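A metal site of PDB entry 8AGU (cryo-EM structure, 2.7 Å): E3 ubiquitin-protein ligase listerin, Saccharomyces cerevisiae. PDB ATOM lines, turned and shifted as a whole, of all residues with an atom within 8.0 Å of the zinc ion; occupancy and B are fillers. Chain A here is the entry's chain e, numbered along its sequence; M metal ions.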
ATOM      1  N   THR A1526      12.057  -0.974   6.738  1.00  0.00           N
ATOM      2  CA  THR A1526      13.506  -1.032   6.854  1.00  0.00           C
ATOM      3  C   THR A1526      13.913  -2.082   7.880  1.00  0.00           C
ATOM      4  O   THR A1526      13.124  -2.472   8.730  1.00  0.00           O
ATOM      5  CB  THR A1526      14.079   0.321   7.296  1.00  0.00           C
ATOM      6  OG1 THR A1526      13.571   0.672   8.590  1.00  0.00           O
ATOM      7  CG2 THR A1526      13.712   1.415   6.301  1.00  0.00           C
ATOM      8  N   CYS A1527      15.161  -2.547   7.796  1.00  0.00           N
ATOM      9  CA  CYS A1527      15.657  -3.523   8.759  1.00  0.00           C
ATOM     10  C   CYS A1527      16.849  -2.960   9.510  1.00  0.00           C
ATOM     11  O   CYS A1527      17.759  -2.384   8.905  1.00  0.00           O
ATOM     12  CB  CYS A1527      16.038  -4.815   8.036  1.00  0.00           C
ATOM     13  SG  CYS A1527      16.756  -6.111   9.061  1.00  0.00           S
ATOM     14  N   PRO A1528      16.864  -3.101  10.839  1.00  0.00           N
ATOM     15  CA  PRO A1528      18.038  -2.639  11.584  1.00  0.00           C
ATOM     16  C   PRO A1528      19.296  -3.418  11.190  1.00  0.00           C
ATOM     17  O   PRO A1528      20.365  -2.818  11.042  1.00  0.00           O
ATOM     18  CB  PRO A1528      17.679  -2.943  13.046  1.00  0.00           C
ATOM     19  CG  PRO A1528      16.187  -2.981  13.063  1.00  0.00           C
ATOM     20  CD  PRO A1528      15.778  -3.530  11.732  1.00  0.00           C
ATOM     21  N   THR A1529      19.168  -4.733  11.029  1.00  0.00           N
ATOM     22  CA  THR A1529      20.309  -5.561  10.643  1.00  0.00           C
ATOM     23  C   THR A1529      20.840  -5.235   9.239  1.00  0.00           C
ATOM     24  O   THR A1529      22.048  -5.154   9.043  1.00  0.00           O
ATOM     25  CB  THR A1529      19.949  -7.051  10.720  1.00  0.00           C
ATOM     26  OG1 THR A1529      19.218  -7.309  11.918  1.00  0.00           O
ATOM     27  CG2 THR A1529      21.207  -7.912  10.704  1.00  0.00           C
ATOM     28  N   CYS A1530      19.947  -5.026   8.274  1.00  0.00           N
ATOM     29  CA  CYS A1530      20.393  -4.787   6.899  1.00  0.00           C
ATOM     30  C   CYS A1530      19.912  -3.479   6.286  1.00  0.00           C
ATOM     31  O   CYS A1530      18.738  -3.132   6.375  1.00  0.00           O
ATOM     32  CB  CYS A1530      20.054  -5.981   5.997  1.00  0.00           C
ATOM     33  SG  CYS A1530      18.293  -6.369   5.833  1.00  0.00           S
ATOM     34  N   LYS A1531      20.816  -2.753   5.632  1.00  0.00           N
ATOM     35  CA  LYS A1531      20.474  -1.436   5.079  1.00  0.00           C
ATOM     36  C   LYS A1531      19.401  -1.396   3.987  1.00  0.00           C
ATOM     37  O   LYS A1531      18.585  -0.471   3.971  1.00  0.00           O
ATOM     38  CB  LYS A1531      21.741  -0.757   4.556  1.00  0.00           C
ATOM     39  CG  LYS A1531      22.813  -0.557   5.620  1.00  0.00           C
ATOM     40  CD  LYS A1531      24.061   0.071   5.030  1.00  0.00           C
ATOM     41  CE  LYS A1531      25.138   0.257   6.097  1.00  0.00           C
ATOM     42  NZ  LYS A1531      26.373   0.870   5.534  1.00  0.00           N
ATOM     43  N   ASN A1532      19.370  -2.374   3.097  1.00  0.00           N
ATOM     44  CA  ASN A1532      18.439  -2.306   1.965  1.00  0.00           C
ATOM     45  C   ASN A1532      16.980  -2.225   2.389  1.00  0.00           C
ATOM     46  O   ASN A1532      16.533  -2.960   3.263  1.00  0.00           O
ATOM     47  CB  ASN A1532      18.643  -3.492   1.030  1.00  0.00           C
ATOM     48  CG  ASN A1532      20.060  -3.581   0.498  1.00  0.00           C
ATOM     49  OD1 ASN A1532      20.364  -4.413  -0.353  1.00  0.00           O
ATOM     50  ND2 ASN A1532      20.933  -2.711   1.000  1.00  0.00           N
ATOM     51  N   PHE A1534      12.737  -2.420   1.999  1.00  0.00           N
ATOM     52  CA  PHE A1534      11.814  -3.407   1.466  1.00  0.00           C
ATOM     53  C   PHE A1534      10.446  -2.801   1.221  1.00  0.00           C
ATOM     54  O   PHE A1534      10.030  -1.905   1.951  1.00  0.00           O
ATOM     55  CB  PHE A1534      11.628  -4.571   2.438  1.00  0.00           C
ATOM     56  CG  PHE A1534      12.918  -5.150   2.949  1.00  0.00           C
ATOM     57  CD1 PHE A1534      13.677  -5.981   2.149  1.00  0.00           C
ATOM     58  CD2 PHE A1534      13.345  -4.872   4.236  1.00  0.00           C
ATOM     59  CE1 PHE A1534      14.857  -6.517   2.621  1.00  0.00           C
ATOM     60  CE2 PHE A1534      14.525  -5.408   4.708  1.00  0.00           C
ATOM     61  CZ  PHE A1534      15.275  -6.229   3.898  1.00  0.00           C
ATOM     62  N   LEU A1539       7.798  -7.147   2.532  1.00  0.00           N
ATOM     63  CA  LEU A1539       8.257  -7.475   3.877  1.00  0.00           C
ATOM     64  C   LEU A1539       7.205  -8.244   4.657  1.00  0.00           C
ATOM     65  O   LEU A1539       7.528  -9.232   5.317  1.00  0.00           O
ATOM     66  CB  LEU A1539       8.640  -6.190   4.622  1.00  0.00           C
ATOM     67  CG  LEU A1539       9.027  -6.333   6.095  1.00  0.00           C
ATOM     68  CD1 LEU A1539      10.412  -5.787   6.352  1.00  0.00           C
ATOM     69  CD2 LEU A1539       7.992  -5.668   6.991  1.00  0.00           C
ATOM     70  N   THR A1550      10.099 -12.634  10.264  1.00  0.00           N
ATOM     71  CA  THR A1550      11.463 -12.662   9.751  1.00  0.00           C
ATOM     72  C   THR A1550      11.763 -11.636   8.652  1.00  0.00           C
ATOM     73  O   THR A1550      10.941 -11.432   7.758  1.00  0.00           O
ATOM     74  CB  THR A1550      11.845 -14.062   9.240  1.00  0.00           C
ATOM     75  OG1 THR A1550      10.830 -14.528   8.346  1.00  0.00           O
ATOM     76  CG2 THR A1550      11.982 -15.023  10.398  1.00  0.00           C
ATOM     77  N   CYS A1551      12.937 -11.024   8.711  1.00  0.00           N
ATOM     78  CA  CYS A1551      13.337 -10.065   7.668  1.00  0.00           C
ATOM     79  C   CYS A1551      13.509 -10.764   6.323  1.00  0.00           C
ATOM     80  O   CYS A1551      13.971 -11.903   6.266  1.00  0.00           O
ATOM     81  CB  CYS A1551      14.640  -9.386   8.082  1.00  0.00           C
ATOM     82  SG  CYS A1551      15.502  -8.463   6.786  1.00  0.00           S
ATOM     83  N   PRO A1552      13.115 -10.108   5.223  1.00  0.00           N
ATOM     84  CA  PRO A1552      13.348 -10.815   3.958  1.00  0.00           C
ATOM     85  C   PRO A1552      14.813 -11.078   3.648  1.00  0.00           C
ATOM     86  O   PRO A1552      15.152 -12.198   3.269  1.00  0.00           O
ATOM     87  CB  PRO A1552      12.764  -9.855   2.920  1.00  0.00           C
ATOM     88  CG  PRO A1552      11.750  -9.055   3.654  1.00  0.00           C
ATOM     89  CD  PRO A1552      12.263  -8.919   5.064  1.00  0.00           C
ATOM     90  N   LEU A1553      15.677 -10.082   3.810  1.00  0.00           N
ATOM     91  CA  LEU A1553      17.108 -10.277   3.594  1.00  0.00           C
ATOM     92  C   LEU A1553      17.802 -11.170   4.608  1.00  0.00           C
ATOM     93  O   LEU A1553      18.669 -11.971   4.245  1.00  0.00           O
ATOM     94  CB  LEU A1553      17.854  -8.954   3.472  1.00  0.00           C
ATOM     95  CG  LEU A1553      17.933  -8.366   2.062  1.00  0.00           C
ATOM     96  CD1 LEU A1553      18.906  -7.190   2.051  1.00  0.00           C
ATOM     97  CD2 LEU A1553      18.377  -9.421   1.070  1.00  0.00           C
ATOM     98  N   CYS A1554      17.449 -11.045   5.877  1.00  0.00           N
ATOM     99  CA  CYS A1554      18.170 -11.793   6.911  1.00  0.00           C
ATOM    100  C   CYS A1554      17.291 -12.622   7.836  1.00  0.00           C
ATOM    101  O   CYS A1554      16.104 -12.339   8.010  1.00  0.00           O
ATOM    102  CB  CYS A1554      19.058 -10.843   7.737  1.00  0.00           C
ATOM    103  SG  CYS A1554      18.174  -9.675   8.795  1.00  0.00           S
ATOM    104  N   ARG A1555      17.867 -13.651   8.442  1.00  0.00           N
ATOM    105  CA  ARG A1555      17.107 -14.540   9.317  1.00  0.00           C
ATOM    106  C   ARG A1555      16.516 -13.832  10.518  1.00  0.00           C
ATOM    107  O   ARG A1555      15.405 -14.151  10.947  1.00  0.00           O
ATOM    108  CB  ARG A1555      17.975 -15.724   9.767  1.00  0.00           C
ATOM    109  CG  ARG A1555      18.588 -16.525   8.630  1.00  0.00           C
ATOM    110  CD  ARG A1555      20.021 -16.102   8.355  1.00  0.00           C
ATOM    111  NE  ARG A1555      20.521 -16.649   7.089  1.00  0.00           N
ATOM    112  CZ  ARG A1555      20.461 -16.005   5.933  1.00  0.00           C
ATOM    113  NH1 ARG A1555      19.928 -14.795   5.865  1.00  0.00           N
ATOM    114  NH2 ARG A1555      20.938 -16.579   4.834  1.00  0.00           N
ATOM    115  N   SER A1556      17.247 -12.871  11.084  1.00  0.00           N
ATOM    116  CA  SER A1556      16.780 -12.214  12.305  1.00  0.00           C
ATOM    117  C   SER A1556      15.429 -11.547  12.137  1.00  0.00           C
ATOM    118  O   SER A1556      15.180 -10.846  11.151  1.00  0.00           O
ATOM    119  CB  SER A1556      17.807 -11.193  12.782  1.00  0.00           C
ATOM    120  OG  SER A1556      17.340 -10.491  13.920  1.00  0.00           O
ATOM    121  N   GLU A1557      14.545 -11.753  13.118  1.00  0.00           N
ATOM    122  CA  GLU A1557      13.210 -11.174  13.054  1.00  0.00           C
ATOM    123  C   GLU A1557      13.144  -9.677  13.321  1.00  0.00           C
ATOM    124  O   GLU A1557      13.972  -9.145  14.052  1.00  0.00           O
ATOM    125  CB  GLU A1557      12.282 -11.901  14.040  1.00  0.00           C
ATOM    126  N   ILE A1558      12.157  -9.001  12.741  1.00  0.00           N
ATOM    127  CA  ILE A1558      11.970  -7.578  13.016  1.00  0.00           C
ATOM    128  C   ILE A1558      10.626  -7.444  13.710  1.00  0.00           C
ATOM    129  O   ILE A1558       9.630  -7.958  13.217  1.00  0.00           O
ATOM    130  CB  ILE A1558      11.906  -6.741  11.727  1.00  0.00           C
ATOM    131  CG1 ILE A1558      12.976  -7.168  10.729  1.00  0.00           C
ATOM    132  CG2 ILE A1558      12.033  -5.262  12.044  1.00  0.00           C
ATOM    133  CD1 ILE A1558      12.883  -6.422   9.423  1.00  0.00           C
HETATM  134 ZN    ZN M   1      17.591  -7.743   7.593  1.00  0.00          ZN
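The side-chain sulfur (SG) of Cys 1527 sits close to the backbone NH (N) of Thr 1529 (3.4 Å). The side-chain sulfur (SG) of Cys 1551 sits close to the backbone NH (N) of Leu 1553, 3.4 Å away. N of Cys 1551 sits at hydrogen-bond distance from O of Ser 1556, 3.3 Å away.
Thr 1529 touches the zinc ion (CB to ZN, 3.98 Å). Within 4 Å of the zinc ion: Cys 1527, Thr 1529, Cys 1530, Cys 1551 and Cys 1554. The nearest printed residue that does not touch the zinc ion is Leu 1553 (4.3 Å).
The zinc ion is bound by SG of Cys 1530 (2.3 Å), SG of Cys 1554 (2.3 Å), SG of Cys 1527 (2.3 Å) and SG of Cys 1551 (2.4 Å). The zinc ion has four donor atoms within binding distance.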
